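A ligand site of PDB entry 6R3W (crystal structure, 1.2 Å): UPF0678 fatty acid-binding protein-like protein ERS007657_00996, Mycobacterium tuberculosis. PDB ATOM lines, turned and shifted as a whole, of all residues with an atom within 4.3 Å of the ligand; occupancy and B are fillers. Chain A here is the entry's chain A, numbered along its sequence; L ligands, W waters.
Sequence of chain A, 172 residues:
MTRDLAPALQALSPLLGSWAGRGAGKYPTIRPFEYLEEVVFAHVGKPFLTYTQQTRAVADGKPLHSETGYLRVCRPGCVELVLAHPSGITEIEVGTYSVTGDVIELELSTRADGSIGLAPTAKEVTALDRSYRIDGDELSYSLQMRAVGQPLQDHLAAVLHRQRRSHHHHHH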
ATOM      1  N   THR A  29     -17.925  20.004  -3.878  1.00  0.00           N
ATOM      2  CA  THR A  29     -19.130  20.826  -3.680  1.00  0.00           C
ATOM      3  C   THR A  29     -18.769  22.266  -3.299  1.00  0.00           C
ATOM      4  O   THR A  29     -19.700  23.073  -3.116  1.00  0.00           O
ATOM      5  CB  THR A  29     -20.002  20.198  -2.586  1.00  0.00           C
ATOM      6  OG1 THR A  29     -19.143  19.997  -1.464  1.00  0.00           O
ATOM      7  CG2 THR A  29     -20.640  18.904  -3.021  1.00  0.00           C
ATOM      8  N   ILE A  30     -17.471  22.564  -3.160  1.00  0.00           N
ATOM      9  CA  ILE A  30     -17.008  23.867  -2.624  1.00  0.00           C
ATOM     10  C   ILE A  30     -15.862  24.394  -3.481  1.00  0.00           C
ATOM     11  O   ILE A  30     -15.331  23.640  -4.303  1.00  0.00           O
ATOM     12  CB  ILE A  30     -16.576  23.753  -1.147  1.00  0.00           C
ATOM     13  CG1 ILE A  30     -15.284  22.923  -1.012  1.00  0.00           C
ATOM     14  CG2 ILE A  30     -17.711  23.205  -0.293  1.00  0.00           C
ATOM     15  CD1 ILE A  30     -14.750  22.808   0.387  1.00  0.00           C
ATOM     16  N   PHE A  33      -9.498  26.198  -0.821  1.00  0.00           N
ATOM     17  CA  PHE A  33      -9.173  27.180   0.232  1.00  0.00           C
ATOM     18  C   PHE A  33      -7.823  26.820   0.851  1.00  0.00           C
ATOM     19  O   PHE A  33      -7.311  25.691   0.658  1.00  0.00           O
ATOM     20  CB  PHE A  33     -10.277  27.236   1.302  1.00  0.00           C
ATOM     21  CG  PHE A  33     -10.520  25.905   1.991  1.00  0.00           C
ATOM     22  CD1 PHE A  33      -9.738  25.499   3.058  1.00  0.00           C
ATOM     23  CD2 PHE A  33     -11.414  24.978   1.438  1.00  0.00           C
ATOM     24  CE1 PHE A  33      -9.880  24.228   3.613  1.00  0.00           C
ATOM     25  CE2 PHE A  33     -11.542  23.709   1.993  1.00  0.00           C
ATOM     26  CZ  PHE A  33     -10.771  23.332   3.078  1.00  0.00           C
ATOM     27  N   TYR A  35      -5.499  27.640   4.791  1.00  0.00           N
ATOM     28  CA  TYR A  35      -5.713  27.971   6.213  1.00  0.00           C
ATOM     29  C   TYR A  35      -4.390  27.939   6.960  1.00  0.00           C
ATOM     30  O   TYR A  35      -3.469  27.185   6.574  1.00  0.00           O
ATOM     31  CB  TYR A  35      -6.737  27.019   6.839  1.00  0.00           C
ATOM     32  CG  TYR A  35      -6.381  25.554   6.787  1.00  0.00           C
ATOM     33  CD1 TYR A  35      -5.740  24.935   7.834  1.00  0.00           C
ATOM     34  CD2 TYR A  35      -6.796  24.763   5.718  1.00  0.00           C
ATOM     35  CE1 TYR A  35      -5.484  23.569   7.816  1.00  0.00           C
ATOM     36  CE2 TYR A  35      -6.520  23.410   5.671  1.00  0.00           C
ATOM     37  CZ  TYR A  35      -5.880  22.797   6.735  1.00  0.00           C
ATOM     38  OH  TYR A  35      -5.662  21.443   6.702  1.00  0.00           O
ATOM     39  N   GLN A  53      -7.474  22.073  18.139  1.00  0.00           N
ATOM     40  CA  GLN A  53      -7.099  22.670  16.856  1.00  0.00           C
ATOM     41  C   GLN A  53      -7.890  23.954  16.703  1.00  0.00           C
ATOM     42  O   GLN A  53      -9.111  23.922  16.894  1.00  0.00           O
ATOM     43  CB  GLN A  53      -7.410  21.708  15.695  1.00  0.00           C
ATOM     44  CG  GLN A  53      -7.125  22.294  14.316  1.00  0.00           C
ATOM     45  CD  GLN A  53      -7.972  21.687  13.239  1.00  0.00           C
ATOM     46  OE1 GLN A  53      -7.494  20.959  12.378  1.00  0.00           O
ATOM     47  NE2 GLN A  53      -9.254  22.017  13.249  1.00  0.00           N
ATOM     48  N   THR A  55      -8.172  26.824  13.371  1.00  0.00           N
ATOM     49  CA  THR A  55      -7.699  27.234  12.034  1.00  0.00           C
ATOM     50  C   THR A  55      -8.287  28.583  11.684  1.00  0.00           C
ATOM     51  O   THR A  55      -9.369  28.931  12.214  1.00  0.00           O
ATOM     52  CB  THR A  55      -8.008  26.194  10.955  1.00  0.00           C
ATOM     53  OG1 THR A  55      -9.422  26.189  10.690  1.00  0.00           O
ATOM     54  CG2 THR A  55      -7.523  24.810  11.349  1.00  0.00           C
ATOM     55  N   LEU A  64     -11.905  29.717  10.888  1.00  0.00           N
ATOM     56  CA  LEU A  64     -12.594  28.758  10.027  1.00  0.00           C
ATOM     57  C   LEU A  64     -13.104  27.609  10.909  1.00  0.00           C
ATOM     58  O   LEU A  64     -13.898  27.886  11.802  1.00  0.00           O
ATOM     59  CB  LEU A  64     -11.631  28.335   8.900  1.00  0.00           C
ATOM     60  CG  LEU A  64     -11.265  29.453   7.913  1.00  0.00           C
ATOM     61  CD1 LEU A  64     -10.247  28.979   6.892  1.00  0.00           C
ATOM     62  CD2 LEU A  64     -12.506  30.012   7.211  1.00  0.00           C
ATOM     63  N   HIS A  65     -12.446  26.484  10.863  1.00  0.00           N
ATOM     64  CA  HIS A  65     -12.797  25.251  11.598  1.00  0.00           C
ATOM     65  C   HIS A  65     -12.000  25.209  12.919  1.00  0.00           C
ATOM     66  O   HIS A  65     -10.845  25.675  12.960  1.00  0.00           O
ATOM     67  CB  HIS A  65     -12.507  24.040  10.703  1.00  0.00           C
ATOM     68  CG  HIS A  65     -12.760  22.724  11.355  1.00  0.00           C
ATOM     69  ND1 HIS A  65     -11.758  21.957  11.929  1.00  0.00           N
ATOM     70  CD2 HIS A  65     -13.909  22.030  11.524  1.00  0.00           C
ATOM     71  CE1 HIS A  65     -12.280  20.819  12.356  1.00  0.00           C
ATOM     72  NE2 HIS A  65     -13.617  20.863  12.140  1.00  0.00           N
ATOM     73  N   GLU A  67     -11.511  21.940  16.221  1.00  0.00           N
ATOM     74  CA  GLU A  67     -11.951  20.657  16.776  1.00  0.00           C
ATOM     75  C   GLU A  67     -11.279  20.482  18.115  1.00  0.00           C
ATOM     76  O   GLU A  67     -10.233  21.088  18.360  1.00  0.00           O
ATOM     77  CB  GLU A  67     -11.697  19.508  15.803  1.00  0.00           C
ATOM     78  CG  GLU A  67     -10.252  19.412  15.338  1.00  0.00           C
ATOM     79  CD  GLU A  67      -9.966  18.418  14.225  1.00  0.00           C
ATOM     80  OE1 GLU A  67     -10.866  18.199  13.363  1.00  0.00           O
ATOM     81  OE2 GLU A  67      -8.836  17.906  14.158  1.00  0.00           O
ATOM     82  N   HIS A  85     -16.847  18.885  16.851  1.00  0.00           N
ATOM     83  CA  HIS A  85     -16.713  19.933  15.811  1.00  0.00           C
ATOM     84  C   HIS A  85     -17.798  20.976  16.000  1.00  0.00           C
ATOM     85  O   HIS A  85     -18.979  20.643  16.246  1.00  0.00           O
ATOM     86  CB  HIS A  85     -16.833  19.335  14.408  1.00  0.00           C
ATOM     87  CG  HIS A  85     -15.817  18.301  14.110  1.00  0.00           C
ATOM     88  ND1 HIS A  85     -14.639  18.609  13.481  1.00  0.00           N
ATOM     89  CD2 HIS A  85     -15.813  16.963  14.304  1.00  0.00           C
ATOM     90  CE1 HIS A  85     -13.905  17.515  13.366  1.00  0.00           C
ATOM     91  NE2 HIS A  85     -14.604  16.503  13.873  1.00  0.00           N
ATOM     92  N   ILE A  89     -21.009  18.226  14.548  1.00  0.00           N
ATOM     93  CA  ILE A  89     -20.603  16.863  14.166  1.00  0.00           C
ATOM     94  C   ILE A  89     -19.694  16.318  15.255  1.00  0.00           C
ATOM     95  O   ILE A  89     -18.795  17.061  15.739  1.00  0.00           O
ATOM     96  CB  ILE A  89     -19.924  16.885  12.783  1.00  0.00           C
ATOM     97  CG1 ILE A  89     -20.907  17.392  11.722  1.00  0.00           C
ATOM     98  CG2 ILE A  89     -19.409  15.499  12.450  1.00  0.00           C
ATOM     99  CD1 ILE A  89     -20.338  17.534  10.351  1.00  0.00           C
ATOM    100  N   LYS A 123     -24.355  19.283   8.191  1.00  0.00           N
ATOM    101  CA  LYS A 123     -24.132  18.672   6.863  1.00  0.00           C
ATOM    102  C   LYS A 123     -23.938  17.160   7.017  1.00  0.00           C
ATOM    103  O   LYS A 123     -23.427  16.709   8.049  1.00  0.00           O
ATOM    104  CB  LYS A 123     -22.926  19.303   6.188  1.00  0.00           C
ATOM    105  CG  LYS A 123     -22.997  20.808   6.009  1.00  0.00           C
ATOM    106  CD  LYS A 123     -23.880  21.227   4.898  1.00  0.00           C
ATOM    107  CE  LYS A 123     -23.789  22.719   4.594  1.00  0.00           C
ATOM    108  NZ  LYS A 123     -22.438  23.093   4.113  1.00  0.00           N
ATOM    109  N   VAL A 125     -22.002  14.235   6.740  1.00  0.00           N
ATOM    110  CA  VAL A 125     -20.673  13.572   6.705  1.00  0.00           C
ATOM    111  C   VAL A 125     -20.873  12.124   7.152  1.00  0.00           C
ATOM    112  O   VAL A 125     -21.509  11.906   8.206  1.00  0.00           O
ATOM    113  CB  VAL A 125     -19.696  14.305   7.617  1.00  0.00           C
ATOM    114  CG1 VAL A 125     -18.359  13.627   7.620  1.00  0.00           C
ATOM    115  CG2 VAL A 125     -19.556  15.770   7.209  1.00  0.00           C
ATOM    116  N   LEU A 128     -14.676   9.740   7.767  1.00  0.00           N
ATOM    117  CA  LEU A 128     -13.439  10.533   7.845  1.00  0.00           C
ATOM    118  C   LEU A 128     -12.263   9.593   8.072  1.00  0.00           C
ATOM    119  O   LEU A 128     -12.366   8.704   8.938  1.00  0.00           O
ATOM    120  CB  LEU A 128     -13.541  11.537   8.988  1.00  0.00           C
ATOM    121  CG  LEU A 128     -14.616  12.610   8.803  1.00  0.00           C
ATOM    122  CD1 LEU A 128     -14.960  13.274  10.125  1.00  0.00           C
ATOM    123  CD2 LEU A 128     -14.206  13.633   7.764  1.00  0.00           C
ATOM    124  N   ARG A 130      -7.953   9.832   8.627  1.00  0.00           N
ATOM    125  CA  ARG A 130      -6.785  10.680   8.922  1.00  0.00           C
ATOM    126  C   ARG A 130      -5.491   9.863   8.828  1.00  0.00           C
ATOM    127  O   ARG A 130      -5.408   8.770   9.410  1.00  0.00           O
ATOM    128  CB  ARG A 130      -6.933  11.309  10.305  1.00  0.00           C
ATOM    129  CG  ARG A 130      -8.025  12.363  10.382  1.00  0.00           C
ATOM    130  CD  ARG A 130      -8.241  12.805  11.816  1.00  0.00           C
ATOM    131  NE  ARG A 130      -9.448  13.596  11.971  1.00  0.00           N
ATOM    132  CZ  ARG A 130      -9.499  14.873  12.334  1.00  0.00           C
ATOM    133  NH1 ARG A 130      -8.387  15.568  12.548  1.00  0.00           N
ATOM    134  NH2 ARG A 130     -10.662  15.458  12.451  1.00  0.00           N
ATOM    135  N   TYR A 141      -0.283  15.932   7.889  1.00  0.00           N
ATOM    136  CA  TYR A 141      -1.442  15.038   7.813  1.00  0.00           C
ATOM    137  C   TYR A 141      -2.180  15.264   6.511  1.00  0.00           C
ATOM    138  O   TYR A 141      -2.117  16.346   5.901  1.00  0.00           O
ATOM    139  CB  TYR A 141      -2.375  15.234   9.008  1.00  0.00           C
ATOM    140  CG  TYR A 141      -3.110  16.552   9.040  1.00  0.00           C
ATOM    141  CD1 TYR A 141      -4.258  16.760   8.298  1.00  0.00           C
ATOM    142  CD2 TYR A 141      -2.631  17.601   9.817  1.00  0.00           C
ATOM    143  CE1 TYR A 141      -4.913  17.976   8.307  1.00  0.00           C
ATOM    144  CE2 TYR A 141      -3.282  18.825   9.854  1.00  0.00           C
ATOM    145  CZ  TYR A 141      -4.427  19.015   9.089  1.00  0.00           C
ATOM    146  OH  TYR A 141      -5.092  20.195   9.100  1.00  0.00           O
ATOM    147  N   LEU A 143      -6.455  14.446   5.467  1.00  0.00           N
ATOM    148  CA  LEU A 143      -7.804  14.011   5.897  1.00  0.00           C
ATOM    149  C   LEU A 143      -8.629  13.784   4.656  1.00  0.00           C
ATOM    150  O   LEU A 143      -8.713  14.671   3.801  1.00  0.00           O
ATOM    151  CB  LEU A 143      -8.420  15.050   6.835  1.00  0.00           C
ATOM    152  CG  LEU A 143      -9.821  14.722   7.336  1.00  0.00           C
ATOM    153  CD1 LEU A 143     -10.042  15.312   8.722  1.00  0.00           C
ATOM    154  CD2 LEU A 143     -10.885  15.234   6.367  1.00  0.00           C
ATOM    155  N   MET A 145     -12.562  12.598   3.344  1.00  0.00           N
ATOM    156  CA  MET A 145     -13.960  12.723   3.789  1.00  0.00           C
ATOM    157  C   MET A 145     -14.878  12.097   2.751  1.00  0.00           C
ATOM    158  O   MET A 145     -14.680  12.306   1.554  1.00  0.00           O
ATOM    159  CB  MET A 145     -14.299  14.191   3.984  1.00  0.00           C
ATOM    160  CG  MET A 145     -15.721  14.440   4.402  1.00  0.00           C
ATOM    161  SD  MET A 145     -15.992  16.129   4.995  1.00  0.00           S
ATOM    162  CE  MET A 145     -15.783  17.077   3.483  1.00  0.00           C
ATOM    163  N   VAL A 148     -21.893  14.481   1.704  1.00  0.00           N
ATOM    164  CA  VAL A 148     -22.731  15.308   0.801  1.00  0.00           C
ATOM    165  C   VAL A 148     -22.672  14.710  -0.626  1.00  0.00           C
ATOM    166  O   VAL A 148     -22.518  15.460  -1.632  1.00  0.00           O
ATOM    167  CB  VAL A 148     -22.357  16.810   0.877  1.00  0.00           C
ATOM    168  CG1 VAL A 148     -22.691  17.396   2.243  1.00  0.00           C
ATOM    169  CG2 VAL A 148     -20.901  17.082   0.514  1.00  0.00           C
ATOM    170  N   HIS A 155     -10.084  16.094   1.675  1.00  0.00           N
ATOM    171  CA  HIS A 155     -10.650  17.422   2.034  1.00  0.00           C
ATOM    172  C   HIS A 155      -9.555  18.350   2.528  1.00  0.00           C
ATOM    173  O   HIS A 155      -9.681  19.547   2.287  1.00  0.00           O
ATOM    174  CB  HIS A 155     -11.785  17.303   3.077  1.00  0.00           C
ATOM    175  CG  HIS A 155     -12.426  18.600   3.505  1.00  0.00           C
ATOM    176  ND1 HIS A 155     -12.798  19.567   2.601  1.00  0.00           N
ATOM    177  CD2 HIS A 155     -12.892  19.026   4.719  1.00  0.00           C
ATOM    178  CE1 HIS A 155     -13.395  20.566   3.251  1.00  0.00           C
ATOM    179  NE2 HIS A 155     -13.433  20.273   4.551  1.00  0.00           N
ATOM    180  N   LEU A 156      -8.557  17.835   3.250  1.00  0.00           N
ATOM    181  CA  LEU A 156      -7.527  18.691   3.892  1.00  0.00           C
ATOM    182  C   LEU A 156      -6.161  18.039   3.731  1.00  0.00           C
ATOM    183  O   LEU A 156      -6.064  16.810   3.869  1.00  0.00           O
ATOM    184  CB  LEU A 156      -7.799  18.859   5.381  1.00  0.00           C
ATOM    185  CG  LEU A 156      -9.200  19.315   5.786  1.00  0.00           C
ATOM    186  CD1 LEU A 156      -9.373  19.088   7.279  1.00  0.00           C
ATOM    187  CD2 LEU A 156      -9.440  20.781   5.429  1.00  0.00           C
HETATM  188  C1  LIG L   1     -16.566  22.705   3.609  1.00  0.00           C
HETATM  189  C2  LIG L   1     -12.589  24.357   5.736  1.00  0.00           C
HETATM  190  C3  LIG L   1     -12.341  20.346   8.500  1.00  0.00           C
HETATM  191  C4  LIG L   1     -16.623  18.935   6.676  1.00  0.00           C
HETATM  192  C5  LIG L   1     -15.498  23.489   3.965  1.00  0.00           C
HETATM  193  C6  LIG L   1     -15.257  24.810   3.448  1.00  0.00           C
HETATM  194  C7  LIG L   1     -14.149  25.267   4.057  1.00  0.00           C
HETATM  195  C8  LIG L   1     -13.690  24.241   4.929  1.00  0.00           C
HETATM  196  C9  LIG L   1     -13.528  26.623   3.880  1.00  0.00           C
HETATM  197  C10 LIG L   1     -16.105  25.530   2.419  1.00  0.00           C
HETATM  198  C11 LIG L   1     -16.868  26.692   3.065  1.00  0.00           C
HETATM  199  C12 LIG L   1     -17.812  26.174   4.103  1.00  0.00           C
HETATM  200  O1  LIG L   1     -17.702  26.578   5.278  1.00  0.00           O
HETATM  201  O2  LIG L   1     -18.724  25.390   3.784  1.00  0.00           O
HETATM  202  C13 LIG L   1     -12.151  23.375   6.638  1.00  0.00           C
HETATM  203  C14 LIG L   1     -10.997  23.517   7.471  1.00  0.00           C
HETATM  204  C15 LIG L   1     -10.882  22.367   8.228  1.00  0.00           C
HETATM  205  C16 LIG L   1     -12.059  21.545   7.879  1.00  0.00           C
HETATM  206  C17 LIG L   1     -10.072  24.715   7.506  1.00  0.00           C
HETATM  207  C18 LIG L   1      -9.846  21.951   9.200  1.00  0.00           C
HETATM  208  C19 LIG L   1      -8.590  22.335   9.076  1.00  0.00           C
HETATM  209  C20 LIG L   1     -13.521  19.634   8.268  1.00  0.00           C
HETATM  210  C21 LIG L   1     -13.899  18.447   8.939  1.00  0.00           C
HETATM  211  C22 LIG L   1     -15.139  18.095   8.477  1.00  0.00           C
HETATM  212  C23 LIG L   1     -15.480  19.018   7.425  1.00  0.00           C
HETATM  213  C24 LIG L   1     -13.063  17.766   9.970  1.00  0.00           C
HETATM  214  C25 LIG L   1     -16.035  17.019   8.944  1.00  0.00           C
HETATM  215  C26 LIG L   1     -16.237  16.767  10.245  1.00  0.00           C
HETATM  216  C27 LIG L   1     -16.923  19.819   5.656  1.00  0.00           C
HETATM  217  C28 LIG L   1     -18.140  19.715   4.828  1.00  0.00           C
HETATM  218  C29 LIG L   1     -18.130  20.750   4.002  1.00  0.00           C
HETATM  219  C30 LIG L   1     -16.884  21.502   4.266  1.00  0.00           C
HETATM  220  C31 LIG L   1     -19.227  18.685   4.981  1.00  0.00           C
HETATM  221  C32 LIG L   1     -19.338  21.284   3.293  1.00  0.00           C
HETATM  222  C33 LIG L   1     -19.389  20.802   1.911  1.00  0.00           C
HETATM  223  C34 LIG L   1     -20.665  21.305   1.234  1.00  0.00           C
HETATM  224  O3  LIG L   1     -21.466  22.211   1.650  1.00  0.00           O
HETATM  225  O4  LIG L   1     -20.925  20.766   0.245  1.00  0.00           O
HETATM  226  N1  LIG L   1     -14.521  23.191   4.898  1.00  0.00           N
HETATM  227  N2  LIG L   1     -12.742  22.193   6.923  1.00  0.00           N
HETATM  228  N3  LIG L   1     -14.465  19.948   7.332  1.00  0.00           N
HETATM  229  N4  LIG L   1     -16.191  20.924   5.289  1.00  0.00           N
HETATM  230 FE1  LIG L   1     -14.484  21.517   6.027  1.00  0.00          FE
HETATM  231  O   HOH W   1     -15.561  22.590   7.539  1.00  0.00           O
HETATM  232  O   HOH W   2      -9.809  19.119  10.875  1.00  0.00           O
HETATM  233  O   HOH W   3     -21.648  24.033  -1.203  1.00  0.00           O
HETATM  234  O   HOH W   4     -20.126  24.093   5.616  1.00  0.00           O
HETATM  235  O   HOH W   5     -15.919  28.642   6.175  1.00  0.00           O
HETATM  236  O   HOH W   6     -17.159  20.215   9.850  1.00  0.00           O
HETATM  237  O   HOH W   7     -23.349  20.093  -0.817  1.00  0.00           O
HETATM  238  O   HOH W   8     -14.357  27.309   0.028  1.00  0.00           O
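The side-chain amino group (NZ) of Lys 123 lies within salt-bridge range of an oxygen (O3) of the ligand, 2.8 Å away.
An iron atom (FE1) of the ligand is bound by a ring nitrogen (NE2) of His 155, at 2.2 Å.
OG1 of Thr 29 sits at hydrogen-bond distance from O4 of the ligand (2.6 Å).
O of Thr 55 lies within hydrogen-bond range of N of Leu 64, at 3.0 Å.
ND1 of His 85 sits at hydrogen-bond distance from NE2 of His 65 (2.8 Å).
The side-chain hydroxyl of Tyr 35 sits at hydrogen-bond distance from the side-chain hydroxyl of Tyr 141 (2.8 Å).
N of His 155 lies within hydrogen-bond range of O of Leu 143 (2.9 Å).
A ring nitrogen (ND1) of His 65 sits at hydrogen-bond distance from the side-chain amide nitrogen (NE2) of Gln 53 (2.8 Å).
The backbone carbonyl oxygen of Leu 156 is in hydrogen-bond range of the backbone NH of Leu 143.
The backbone carbonyl oxygen (O) of His 65 lies within hydrogen-bond range of the side-chain hydroxyl (OG1) of Thr 55 (2.7 Å).
The backbone carbonyl oxygen of Glu 67 lies within hydrogen-bond range of the backbone NH of Gln 53 (2.9 Å).
CD1 of Ile 30 touches C10 of the ligand, at 3.7 Å.
Phe 33 touches the ligand.
CE1 of Tyr 35 touches C19 of the ligand, 3.6 Å away.
OE1 of Gln 53 touches C19 of the ligand (3.7 Å).
Thr 55 touches the ligand.
ND1 of His 65 touches C18 of the ligand, 3.3 Å away.
CE1 of His 85 touches C24 of the ligand, 3.5 Å away.
Val 125 touches the ligand (CG2 to C31, 3.7 Å).
Leu 128 touches the ligand.
SD of Met 145 touches C4 of the ligand (3.3 Å).
Val 148 touches the ligand (CG2 to O4, 3.7 Å).
CD1 of Leu 156 touches C3 of the ligand, 3.4 Å away.
Of the 21 residues printed, 15 come within 4 Å of the ligand.
Along chain A the residues within 4 Å of the ligand span positions 29 to 156.
The nearest printed residue that does not touch the ligand is Glu 67 (4.1 Å).
Water W4 lies within hydrogen-bond range of an oxygen (O2) of the ligand (2.6 Å) and the side-chain amino group of Lys 123 (2.9 Å).
Water W2 lies within hydrogen-bond range of OE1 of Glu 67 and OE1 of Gln 53.
Water W3 bridges the backbone carbonyl oxygen (O) of Thr 29 (2.9 Å) and an oxygen (O3) of the ligand (3.4 Å).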
